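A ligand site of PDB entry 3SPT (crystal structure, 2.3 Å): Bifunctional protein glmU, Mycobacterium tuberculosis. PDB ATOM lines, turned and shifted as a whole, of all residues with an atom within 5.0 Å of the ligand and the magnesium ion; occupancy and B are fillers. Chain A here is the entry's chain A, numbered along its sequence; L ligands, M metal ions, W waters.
O of Leu 18 lies within hydrogen-bond range of O9 of the ligand, 3.2 Å away.
The side-chain hydroxyl of Thr 95 lies within hydrogen-bond range of an oxygen (O6) of the ligand.
N of Leu 93 lies within hydrogen-bond range of O8 of the ligand (3.4 Å).
The backbone NH (N) of Ala 19 sits close to an oxygen (O9) of the ligand, at 3.5 Å.
O14 of the ligand lies close to NZ of Lys 32 (3.8 Å).
O7 of the ligand is in hydrogen-bond range of N of Ala 20.
An oxygen (O2) of the ligand is in hydrogen-bond range of the side-chain amide nitrogen (ND2) of Asn 187, 2.7 Å away.
NH2 of Arg 25 is in salt-bridge range of O17 of the ligand, 3.6 Å away.
OE1 of Glu 172 lies within hydrogen-bond range of N1 of the ligand (2.6 Å).
The backbone NH of Gly 157 is in hydrogen-bond range of an oxygen (O3) of the ligand (2.8 Å).
A nitrogen (N3) of the ligand lies within hydrogen-bond range of the side-chain amide oxygen (OE1) of Gln 89 (2.7 Å).
O9 of the ligand is in hydrogen-bond range of N of Gly 21 (3.3 Å).
An oxygen (O8) of the ligand lies within hydrogen-bond range of the backbone NH (N) of Gly 94, 2.7 Å away.
An oxygen (O3) of the ligand lies within hydrogen-bond range of the backbone carbonyl oxygen of Asn 187 (2.4 Å).
The backbone carbonyl oxygen (O) of Pro 92 sits close to an oxygen (O8) of the ligand, at 3.4 Å.
Ala 98 touches the ligand (CB to O7, 3.3 Å).
Ser 118 touches the ligand.
CA of Tyr 156 touches O3 of the ligand (3.4 Å).
O of Ala 188 touches C6 of the ligand, 3.8 Å away.
Tyr 215 touches the ligand (CD1 to C8, 3.6 Å).
Thr 217 touches the ligand (CG2 to O2, 3.2 Å).
Hydrophobic or aromatic side chains within 4 Å of the ligand: Leu 18, Ala 20, Pro 92, Ala 98, Tyr 156 and Tyr 215.
Along chain A the residues within 4 Å of the ligand span positions 18 to 245.
The backbone carbonyl oxygen (O) of Val 61 lies within hydrogen-bond range of the backbone NH (N) of Ala 20 (3.2 Å).
N of Val 244 is in hydrogen-bond range of O of Asp 120, at 3.0 Å.
NZ of Lys 32 lies close to O of Val 244 (3.5 Å).
The side-chain amide nitrogen of Asn 187 is in hydrogen-bond range of the side-chain hydroxyl of Tyr 191, 2.9 Å away.
The backbone carbonyl oxygen (O) of Val 61 sits at hydrogen-bond distance from the backbone NH (N) of Ala 19 (2.8 Å).
N of Asn 187 sits at hydrogen-bond distance from O of Gly 157, at 2.8 Å.
The side-chain hydroxyl (OH) of Tyr 156 sits at hydrogen-bond distance from the backbone NH (N) of Gly 243, at 3.1 Å.
The side-chain amide nitrogen (NE2) of Gln 89 lies close to the backbone NH (N) of Ala 98, 3.2 Å away.
Water W2 lies within hydrogen-bond range of O5 of the ligand (2.7 Å) and ND2 of Asn 245 (3.3 Å).
Water W5 lies within hydrogen-bond range of O5 of the ligand (2.8 Å) and OD1 of Asp 120 (2.8 Å).
Water W1 lies within hydrogen-bond range of O17 of the ligand (2.5 Å) and O of Gly 155 (2.8 Å).
Water W3 lies within hydrogen-bond range of O of Ala 188 (2.8 Å), O5 of the ligand (2.9 Å), OG1 of Thr 121 (2.9 Å) and N of Gly 243 (3.4 Å).
NZ of Lys 32 touches the magnesium ion, 3.9 Å away.
Within 4 Å of the magnesium ion: Lys 32, Asp 120 and Asn 245.
The nearest printed residue that does not touch the magnesium ion is Val 244 (4.5 Å).
The magnesium ion is bound by O14 of the ligand (2.1 Å).
Water W2 is bound to the magnesium ion (2.2 Å).
OD1 of Asn 245 is bound to the magnesium ion, at 2.2 Å.
The side-chain carboxylate (OD2) of Asp 120 is bound to the magnesium ion.
The magnesium ion is bound by water W5 (2.2 Å).
O16 of the ligand binds the magnesium ion.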
ATOM      1  N   LEU A  18     -32.832  24.804  30.358  1.00  0.00           N
ATOM      2  CA  LEU A  18     -31.891  24.311  29.327  1.00  0.00           C
ATOM      3  C   LEU A  18     -30.820  23.493  29.993  1.00  0.00           C
ATOM      4  O   LEU A  18     -30.101  23.986  30.867  1.00  0.00           O
ATOM      5  CB  LEU A  18     -31.210  25.470  28.624  1.00  0.00           C
ATOM      6  CG  LEU A  18     -32.135  26.585  28.211  1.00  0.00           C
ATOM      7  CD1 LEU A  18     -31.224  27.570  27.455  1.00  0.00           C
ATOM      8  CD2 LEU A  18     -33.280  25.994  27.244  1.00  0.00           C
ATOM      9  N   ALA A  19     -30.715  22.220  29.620  1.00  0.00           N
ATOM     10  CA  ALA A  19     -29.781  21.350  30.262  1.00  0.00           C
ATOM     11  C   ALA A  19     -29.202  20.412  29.224  1.00  0.00           C
ATOM     12  O   ALA A  19     -28.890  19.278  29.536  1.00  0.00           O
ATOM     13  CB  ALA A  19     -30.529  20.575  31.293  1.00  0.00           C
ATOM     14  N   ALA A  20     -29.098  20.859  27.983  1.00  0.00           N
ATOM     15  CA  ALA A  20     -28.653  19.961  26.908  1.00  0.00           C
ATOM     16  C   ALA A  20     -27.221  20.264  26.372  1.00  0.00           C
ATOM     17  O   ALA A  20     -26.796  19.702  25.344  1.00  0.00           O
ATOM     18  CB  ALA A  20     -29.662  19.993  25.807  1.00  0.00           C
ATOM     19  N   GLY A  21     -26.470  21.135  27.076  1.00  0.00           N
ATOM     20  CA  GLY A  21     -25.144  21.541  26.608  1.00  0.00           C
ATOM     21  C   GLY A  21     -24.183  20.444  26.918  1.00  0.00           C
ATOM     22  O   GLY A  21     -24.509  19.559  27.713  1.00  0.00           O
ATOM     23  N   ARG A  25     -16.252  21.973  30.142  1.00  0.00           N
ATOM     24  CA  ARG A  25     -15.331  22.490  31.157  1.00  0.00           C
ATOM     25  C   ARG A  25     -15.381  21.737  32.543  1.00  0.00           C
ATOM     26  O   ARG A  25     -14.503  21.932  33.389  1.00  0.00           O
ATOM     27  CB  ARG A  25     -15.459  24.036  31.290  1.00  0.00           C
ATOM     28  CG  ARG A  25     -15.151  24.853  29.998  1.00  0.00           C
ATOM     29  CD  ARG A  25     -15.739  26.343  30.012  1.00  0.00           C
ATOM     30  NE  ARG A  25     -17.197  26.482  30.246  1.00  0.00           N
ATOM     31  CZ  ARG A  25     -18.107  26.924  29.368  1.00  0.00           C
ATOM     32  NH1 ARG A  25     -17.767  27.270  28.122  1.00  0.00           N
ATOM     33  NH2 ARG A  25     -19.388  26.999  29.711  1.00  0.00           N
ATOM     34  N   LYS A  32     -22.953  17.243  33.548  1.00  0.00           N
ATOM     35  CA  LYS A  32     -22.917  18.387  34.469  1.00  0.00           C
ATOM     36  C   LYS A  32     -24.120  18.406  35.398  1.00  0.00           C
ATOM     37  O   LYS A  32     -23.997  18.153  36.599  1.00  0.00           O
ATOM     38  CB  LYS A  32     -22.840  19.696  33.688  1.00  0.00           C
ATOM     39  CG  LYS A  32     -22.792  20.937  34.552  1.00  0.00           C
ATOM     40  CD  LYS A  32     -22.143  22.106  33.824  1.00  0.00           C
ATOM     41  CE  LYS A  32     -23.176  22.931  33.080  1.00  0.00           C
ATOM     42  NZ  LYS A  32     -22.541  23.960  32.212  1.00  0.00           N
ATOM     43  N   VAL A  61     -34.890  20.747  28.664  1.00  0.00           N
ATOM     44  CA  VAL A  61     -34.368  20.443  27.359  1.00  0.00           C
ATOM     45  C   VAL A  61     -33.118  19.668  27.615  1.00  0.00           C
ATOM     46  O   VAL A  61     -32.185  20.188  28.289  1.00  0.00           O
ATOM     47  CB  VAL A  61     -33.997  21.727  26.652  1.00  0.00           C
ATOM     48  CG1 VAL A  61     -33.387  21.435  25.247  1.00  0.00           C
ATOM     49  CG2 VAL A  61     -35.240  22.605  26.529  1.00  0.00           C
ATOM     50  N   GLN A  89     -32.840  18.163  22.234  1.00  0.00           N
ATOM     51  CA  GLN A  89     -32.040  18.979  21.391  1.00  0.00           C
ATOM     52  C   GLN A  89     -30.978  18.048  20.884  1.00  0.00           C
ATOM     53  O   GLN A  89     -30.054  17.666  21.634  1.00  0.00           O
ATOM     54  CB  GLN A  89     -31.407  20.149  22.176  1.00  0.00           C
ATOM     55  CG  GLN A  89     -30.604  21.028  21.213  1.00  0.00           C
ATOM     56  CD  GLN A  89     -29.760  22.125  21.844  1.00  0.00           C
ATOM     57  OE1 GLN A  89     -29.123  21.936  22.885  1.00  0.00           O
ATOM     58  NE2 GLN A  89     -29.749  23.270  21.209  1.00  0.00           N
ATOM     59  N   PRO A  92     -25.952  20.364  20.220  1.00  0.00           N
ATOM     60  CA  PRO A  92     -25.906  21.616  21.026  1.00  0.00           C
ATOM     61  C   PRO A  92     -25.554  22.846  20.179  1.00  0.00           C
ATOM     62  O   PRO A  92     -24.444  23.348  20.188  1.00  0.00           O
ATOM     63  CB  PRO A  92     -24.830  21.310  22.068  1.00  0.00           C
ATOM     64  CG  PRO A  92     -23.901  20.345  21.349  1.00  0.00           C
ATOM     65  CD  PRO A  92     -24.823  19.462  20.533  1.00  0.00           C
ATOM     66  N   LEU A  93     -26.546  23.368  19.473  1.00  0.00           N
ATOM     67  CA  LEU A  93     -26.285  24.418  18.532  1.00  0.00           C
ATOM     68  C   LEU A  93     -26.400  25.772  19.184  1.00  0.00           C
ATOM     69  O   LEU A  93     -26.321  26.783  18.491  1.00  0.00           O
ATOM     70  CB  LEU A  93     -27.306  24.312  17.408  1.00  0.00           C
ATOM     71  CG  LEU A  93     -26.818  23.607  16.123  1.00  0.00           C
ATOM     72  CD1 LEU A  93     -25.596  22.751  16.249  1.00  0.00           C
ATOM     73  CD2 LEU A  93     -27.974  22.836  15.478  1.00  0.00           C
ATOM     74  N   GLY A  94     -26.604  25.824  20.496  1.00  0.00           N
ATOM     75  CA  GLY A  94     -26.683  27.098  21.156  1.00  0.00           C
ATOM     76  C   GLY A  94     -27.905  27.242  22.050  1.00  0.00           C
ATOM     77  O   GLY A  94     -28.913  26.501  21.895  1.00  0.00           O
ATOM     78  N   THR A  95     -27.837  28.194  22.967  1.00  0.00           N
ATOM     79  CA  THR A  95     -28.920  28.367  23.914  1.00  0.00           C
ATOM     80  C   THR A  95     -30.199  28.831  23.197  1.00  0.00           C
ATOM     81  O   THR A  95     -31.305  28.581  23.639  1.00  0.00           O
ATOM     82  CB  THR A  95     -28.529  29.366  25.038  1.00  0.00           C
ATOM     83  OG1 THR A  95     -28.112  30.605  24.433  1.00  0.00           O
ATOM     84  CG2 THR A  95     -27.414  28.844  25.862  1.00  0.00           C
ATOM     85  N   ALA A  98     -31.634  25.755  21.749  1.00  0.00           N
ATOM     86  CA  ALA A  98     -32.190  24.982  22.865  1.00  0.00           C
ATOM     87  C   ALA A  98     -33.587  25.472  23.225  1.00  0.00           C
ATOM     88  O   ALA A  98     -34.471  24.676  23.475  1.00  0.00           O
ATOM     89  CB  ALA A  98     -31.261  25.017  24.133  1.00  0.00           C
ATOM     90  N   SER A 118     -31.310  28.117  33.243  1.00  0.00           N
ATOM     91  CA  SER A 118     -30.342  27.023  33.008  1.00  0.00           C
ATOM     92  C   SER A 118     -30.397  25.908  33.995  1.00  0.00           C
ATOM     93  O   SER A 118     -30.785  26.099  35.139  1.00  0.00           O
ATOM     94  CB  SER A 118     -28.932  27.528  32.995  1.00  0.00           C
ATOM     95  OG  SER A 118     -28.856  28.683  32.143  1.00  0.00           O
ATOM     96  N   GLY A 119     -29.968  24.729  33.610  1.00  0.00           N
ATOM     97  CA  GLY A 119     -29.828  23.707  34.605  1.00  0.00           C
ATOM     98  C   GLY A 119     -28.593  23.840  35.528  1.00  0.00           C
ATOM     99  O   GLY A 119     -28.438  23.013  36.441  1.00  0.00           O
ATOM    100  N   ASP A 120     -27.732  24.844  35.298  1.00  0.00           N
ATOM    101  CA  ASP A 120     -26.544  25.053  36.118  1.00  0.00           C
ATOM    102  C   ASP A 120     -26.506  26.312  37.061  1.00  0.00           C
ATOM    103  O   ASP A 120     -25.430  26.833  37.361  1.00  0.00           O
ATOM    104  CB  ASP A 120     -25.274  24.942  35.245  1.00  0.00           C
ATOM    105  CG  ASP A 120     -25.138  26.052  34.260  1.00  0.00           C
ATOM    106  OD1 ASP A 120     -25.914  27.028  34.251  1.00  0.00           O
ATOM    107  OD2 ASP A 120     -24.199  25.974  33.427  1.00  0.00           O
ATOM    108  N   THR A 121     -27.678  26.761  37.501  1.00  0.00           N
ATOM    109  CA  THR A 121     -27.853  27.886  38.354  1.00  0.00           C
ATOM    110  C   THR A 121     -28.533  27.378  39.606  1.00  0.00           C
ATOM    111  O   THR A 121     -29.665  27.773  39.917  1.00  0.00           O
ATOM    112  CB  THR A 121     -28.640  28.940  37.633  1.00  0.00           C
ATOM    113  OG1 THR A 121     -27.758  29.533  36.660  1.00  0.00           O
ATOM    114  CG2 THR A 121     -29.045  30.076  38.535  1.00  0.00           C
ATOM    115  N   GLY A 155     -16.427  35.002  31.785  1.00  0.00           N
ATOM    116  CA  GLY A 155     -17.289  33.913  31.322  1.00  0.00           C
ATOM    117  C   GLY A 155     -18.731  34.259  31.042  1.00  0.00           C
ATOM    118  O   GLY A 155     -19.379  33.620  30.222  1.00  0.00           O
ATOM    119  N   TYR A 156     -19.243  35.270  31.713  1.00  0.00           N
ATOM    120  CA  TYR A 156     -20.605  35.681  31.623  1.00  0.00           C
ATOM    121  C   TYR A 156     -20.885  36.640  30.427  1.00  0.00           C
ATOM    122  O   TYR A 156     -19.978  37.323  29.953  1.00  0.00           O
ATOM    123  CB  TYR A 156     -20.904  36.402  32.913  1.00  0.00           C
ATOM    124  CG  TYR A 156     -21.173  35.580  34.185  1.00  0.00           C
ATOM    125  CD1 TYR A 156     -22.524  35.230  34.578  1.00  0.00           C
ATOM    126  CD2 TYR A 156     -20.118  35.244  35.089  1.00  0.00           C
ATOM    127  CE1 TYR A 156     -22.822  34.531  35.784  1.00  0.00           C
ATOM    128  CE2 TYR A 156     -20.405  34.536  36.298  1.00  0.00           C
ATOM    129  CZ  TYR A 156     -21.759  34.193  36.625  1.00  0.00           C
ATOM    130  OH  TYR A 156     -22.009  33.503  37.785  1.00  0.00           O
ATOM    131  N   GLY A 157     -22.143  36.694  29.925  1.00  0.00           N
ATOM    132  CA  GLY A 157     -22.525  37.768  28.974  1.00  0.00           C
ATOM    133  C   GLY A 157     -22.499  39.149  29.701  1.00  0.00           C
ATOM    134  O   GLY A 157     -22.870  39.237  30.883  1.00  0.00           O
ATOM    135  N   ILE A 170     -26.769  42.165  25.118  1.00  0.00           N
ATOM    136  CA  ILE A 170     -25.897  41.370  25.945  1.00  0.00           C
ATOM    137  C   ILE A 170     -24.762  40.881  25.030  1.00  0.00           C
ATOM    138  O   ILE A 170     -25.020  40.455  23.897  1.00  0.00           O
ATOM    139  CB  ILE A 170     -26.637  40.165  26.506  1.00  0.00           C
ATOM    140  CG1 ILE A 170     -27.749  40.632  27.472  1.00  0.00           C
ATOM    141  CG2 ILE A 170     -25.657  39.208  27.191  1.00  0.00           C
ATOM    142  CD1 ILE A 170     -28.695  39.459  27.871  1.00  0.00           C
ATOM    143  N   GLU A 172     -21.353  38.292  24.658  1.00  0.00           N
ATOM    144  CA  GLU A 172     -20.747  37.061  25.284  1.00  0.00           C
ATOM    145  C   GLU A 172     -19.260  37.241  25.561  1.00  0.00           C
ATOM    146  O   GLU A 172     -18.621  37.956  24.851  1.00  0.00           O
ATOM    147  CB  GLU A 172     -20.976  35.814  24.411  1.00  0.00           C
ATOM    148  CG  GLU A 172     -22.417  35.310  24.403  1.00  0.00           C
ATOM    149  CD  GLU A 172     -22.930  35.066  25.813  1.00  0.00           C
ATOM    150  OE1 GLU A 172     -22.481  34.088  26.463  1.00  0.00           O
ATOM    151  OE2 GLU A 172     -23.765  35.861  26.254  1.00  0.00           O
ATOM    152  N   ASN A 187     -25.096  38.914  32.566  1.00  0.00           N
ATOM    153  CA  ASN A 187     -26.366  38.168  32.305  1.00  0.00           C
ATOM    154  C   ASN A 187     -26.446  36.915  33.151  1.00  0.00           C
ATOM    155  O   ASN A 187     -25.531  36.085  33.064  1.00  0.00           O
ATOM    156  CB  ASN A 187     -26.394  37.788  30.847  1.00  0.00           C
ATOM    157  CG  ASN A 187     -27.600  36.943  30.474  1.00  0.00           C
ATOM    158  OD1 ASN A 187     -28.671  37.104  31.010  1.00  0.00           O
ATOM    159  ND2 ASN A 187     -27.414  36.059  29.490  1.00  0.00           N
ATOM    160  N   ALA A 188     -27.522  36.782  33.934  1.00  0.00           N
ATOM    161  CA  ALA A 188     -27.706  35.591  34.767  1.00  0.00           C
ATOM    162  C   ALA A 188     -28.206  34.379  33.987  1.00  0.00           C
ATOM    163  O   ALA A 188     -28.149  33.226  34.498  1.00  0.00           O
ATOM    164  CB  ALA A 188     -28.662  35.873  35.897  1.00  0.00           C
ATOM    165  N   GLY A 189     -28.690  34.620  32.768  1.00  0.00           N
ATOM    166  CA  GLY A 189     -29.212  33.579  31.904  1.00  0.00           C
ATOM    167  C   GLY A 189     -30.610  33.187  32.365  1.00  0.00           C
ATOM    168  O   GLY A 189     -30.957  32.033  32.289  1.00  0.00           O
ATOM    169  N   TYR A 191     -34.573  34.552  32.164  1.00  0.00           N
ATOM    170  CA  TYR A 191     -35.351  35.449  31.363  1.00  0.00           C
ATOM    171  C   TYR A 191     -36.864  35.189  31.542  1.00  0.00           C
ATOM    172  O   TYR A 191     -37.297  34.077  31.770  1.00  0.00           O
ATOM    173  CB  TYR A 191     -35.048  35.221  29.903  1.00  0.00           C
ATOM    174  CG  TYR A 191     -33.607  35.113  29.497  1.00  0.00           C
ATOM    175  CD1 TYR A 191     -32.894  33.923  29.660  1.00  0.00           C
ATOM    176  CD2 TYR A 191     -32.968  36.170  28.874  1.00  0.00           C
ATOM    177  CE1 TYR A 191     -31.583  33.813  29.245  1.00  0.00           C
ATOM    178  CE2 TYR A 191     -31.627  36.055  28.439  1.00  0.00           C
ATOM    179  CZ  TYR A 191     -30.955  34.885  28.637  1.00  0.00           C
ATOM    180  OH  TYR A 191     -29.676  34.793  28.162  1.00  0.00           O
ATOM    181  N   TYR A 215     -27.278  32.174  19.742  1.00  0.00           N
ATOM    182  CA  TYR A 215     -27.223  32.734  21.134  1.00  0.00           C
ATOM    183  C   TYR A 215     -28.576  33.171  21.546  1.00  0.00           C
ATOM    184  O   TYR A 215     -29.166  34.002  20.876  1.00  0.00           O
ATOM    185  CB  TYR A 215     -26.342  33.999  21.202  1.00  0.00           C
ATOM    186  CG  TYR A 215     -24.838  33.797  21.077  1.00  0.00           C
ATOM    187  CD1 TYR A 215     -24.251  32.580  21.367  1.00  0.00           C
ATOM    188  CD2 TYR A 215     -24.003  34.864  20.759  1.00  0.00           C
ATOM    189  CE1 TYR A 215     -22.846  32.392  21.300  1.00  0.00           C
ATOM    190  CE2 TYR A 215     -22.609  34.681  20.680  1.00  0.00           C
ATOM    191  CZ  TYR A 215     -22.041  33.439  20.937  1.00  0.00           C
ATOM    192  OH  TYR A 215     -20.676  33.228  20.846  1.00  0.00           O
ATOM    193  N   LEU A 216     -29.089  32.667  22.658  1.00  0.00           N
ATOM    194  CA  LEU A 216     -30.327  33.247  23.231  1.00  0.00           C
ATOM    195  C   LEU A 216     -30.135  34.713  23.575  1.00  0.00           C
ATOM    196  O   LEU A 216     -31.097  35.486  23.576  1.00  0.00           O
ATOM    197  CB  LEU A 216     -30.731  32.508  24.494  1.00  0.00           C
ATOM    198  CG  LEU A 216     -32.017  32.928  25.168  1.00  0.00           C
ATOM    199  CD1 LEU A 216     -33.197  32.868  24.197  1.00  0.00           C
ATOM    200  CD2 LEU A 216     -32.230  31.990  26.345  1.00  0.00           C
ATOM    201  N   THR A 217     -28.883  35.117  23.812  1.00  0.00           N
ATOM    202  CA  THR A 217     -28.588  36.462  24.329  1.00  0.00           C
ATOM    203  C   THR A 217     -28.822  37.517  23.268  1.00  0.00           C
ATOM    204  O   THR A 217     -29.168  38.636  23.591  1.00  0.00           O
ATOM    205  CB  THR A 217     -27.150  36.554  24.842  1.00  0.00           C
ATOM    206  OG1 THR A 217     -26.333  35.853  23.908  1.00  0.00           O
ATOM    207  CG2 THR A 217     -26.996  35.916  26.239  1.00  0.00           C
ATOM    208  N   GLY A 243     -23.658  30.911  38.013  1.00  0.00           N
ATOM    209  CA  GLY A 243     -23.613  29.668  37.299  1.00  0.00           C
ATOM    210  C   GLY A 243     -22.475  28.797  37.665  1.00  0.00           C
ATOM    211  O   GLY A 243     -21.529  29.252  38.245  1.00  0.00           O
ATOM    212  N   VAL A 244     -22.563  27.548  37.220  1.00  0.00           N
ATOM    213  CA  VAL A 244     -21.572  26.546  37.377  1.00  0.00           C
ATOM    214  C   VAL A 244     -21.157  25.862  35.989  1.00  0.00           C
ATOM    215  O   VAL A 244     -21.839  24.926  35.470  1.00  0.00           O
ATOM    216  CB  VAL A 244     -22.094  25.491  38.299  1.00  0.00           C
ATOM    217  CG1 VAL A 244     -21.070  24.284  38.415  1.00  0.00           C
ATOM    218  CG2 VAL A 244     -22.464  26.101  39.650  1.00  0.00           C
ATOM    219  N   ASN A 245     -20.028  26.329  35.435  1.00  0.00           N
ATOM    220  CA  ASN A 245     -19.461  25.689  34.255  1.00  0.00           C
ATOM    221  C   ASN A 245     -18.281  24.734  34.470  1.00  0.00           C
ATOM    222  O   ASN A 245     -17.915  24.032  33.536  1.00  0.00           O
ATOM    223  CB  ASN A 245     -19.063  26.762  33.231  1.00  0.00           C
ATOM    224  CG  ASN A 245     -20.250  27.589  32.785  1.00  0.00           C
ATOM    225  OD1 ASN A 245     -21.392  27.137  32.833  1.00  0.00           O
ATOM    226  ND2 ASN A 245     -19.978  28.794  32.320  1.00  0.00           N
HETATM  227  C1  LIG L   1     -24.650  31.640  29.440  1.00  0.00           C
HETATM  228  C2  LIG L   1     -25.030  32.897  28.667  1.00  0.00           C
HETATM  229  C3  LIG L   1     -24.435  34.136  29.330  1.00  0.00           C
HETATM  230  C4  LIG L   1     -24.733  34.153  30.826  1.00  0.00           C
HETATM  231  C5  LIG L   1     -24.381  32.823  31.466  1.00  0.00           C
HETATM  232  C6  LIG L   1     -24.748  32.807  32.942  1.00  0.00           C
HETATM  233  C7  LIG L   1     -25.398  32.511  26.304  1.00  0.00           C
HETATM  234  C8  LIG L   1     -24.853  32.745  24.918  1.00  0.00           C
HETATM  235  N1  LIG L   1     -24.562  32.790  27.300  1.00  0.00           N
HETATM  236  O1  LIG L   1     -23.235  31.450  29.395  1.00  0.00           O
HETATM  237  O2  LIG L   1     -24.987  35.311  28.714  1.00  0.00           O
HETATM  238  O3  LIG L   1     -23.986  35.205  31.441  1.00  0.00           O
HETATM  239  O4  LIG L   1     -25.069  31.768  30.799  1.00  0.00           O
HETATM  240  O5  LIG L   1     -24.639  31.476  33.455  1.00  0.00           O
HETATM  241  O6  LIG L   1     -26.520  32.094  26.498  1.00  0.00           O
HETATM  242  N2  LIG L   1     -27.481  24.607  26.582  1.00  0.00           N
HETATM  243  C9  LIG L   1     -28.234  23.847  25.657  1.00  0.00           C
HETATM  244  N3  LIG L   1     -27.877  23.783  24.370  1.00  0.00           N
HETATM  245  C10 LIG L   1     -26.787  24.441  23.937  1.00  0.00           C
HETATM  246  C11 LIG L   1     -26.025  25.197  24.821  1.00  0.00           C
HETATM  247  C12 LIG L   1     -26.391  25.268  26.159  1.00  0.00           C
HETATM  248  O7  LIG L   1     -29.247  23.234  26.051  1.00  0.00           O
HETATM  249  O8  LIG L   1     -26.469  24.374  22.737  1.00  0.00           O
HETATM  250  C13 LIG L   1     -27.874  24.669  27.987  1.00  0.00           C
HETATM  251  C14 LIG L   1     -26.783  24.064  28.851  1.00  0.00           C
HETATM  252  O9  LIG L   1     -27.326  22.983  29.622  1.00  0.00           O
HETATM  253  C15 LIG L   1     -26.313  25.170  29.787  1.00  0.00           C
HETATM  254  C16 LIG L   1     -27.153  26.391  29.442  1.00  0.00           C
HETATM  255  O10 LIG L   1     -28.035  26.030  28.380  1.00  0.00           O
HETATM  256  O11 LIG L   1     -26.568  24.786  31.143  1.00  0.00           O
HETATM  257  C17 LIG L   1     -26.266  27.552  28.994  1.00  0.00           C
HETATM  258  O12 LIG L   1     -25.083  27.032  28.389  1.00  0.00           O
HETATM  259  P1  LIG L   1     -23.625  27.455  28.928  1.00  0.00           P
HETATM  260  O13 LIG L   1     -22.586  26.880  28.001  1.00  0.00           O
HETATM  261  O14 LIG L   1     -23.573  27.162  30.411  1.00  0.00           O
HETATM  262  O15 LIG L   1     -23.634  29.063  28.740  1.00  0.00           O
HETATM  263  P2  LIG L   1     -22.604  29.984  29.553  1.00  0.00           P
HETATM  264  O16 LIG L   1     -22.656  29.597  31.007  1.00  0.00           O
HETATM  265  O17 LIG L   1     -21.276  29.960  28.818  1.00  0.00           O
HETATM  266 MG    MG M   1     -23.437  27.770  32.436  1.00  0.00          MG
HETATM  267  O   HOH W   1     -19.129  30.936  29.528  1.00  0.00           O
HETATM  268  O   HOH W   2     -22.906  29.439  33.697  1.00  0.00           O
HETATM  269  O   HOH W   3     -26.112  31.837  35.887  1.00  0.00           O
HETATM  270  O   HOH W   4     -23.035  26.839  24.850  1.00  0.00           O
HETATM  271  O   HOH W   5     -25.284  28.991  32.292  1.00  0.00           O
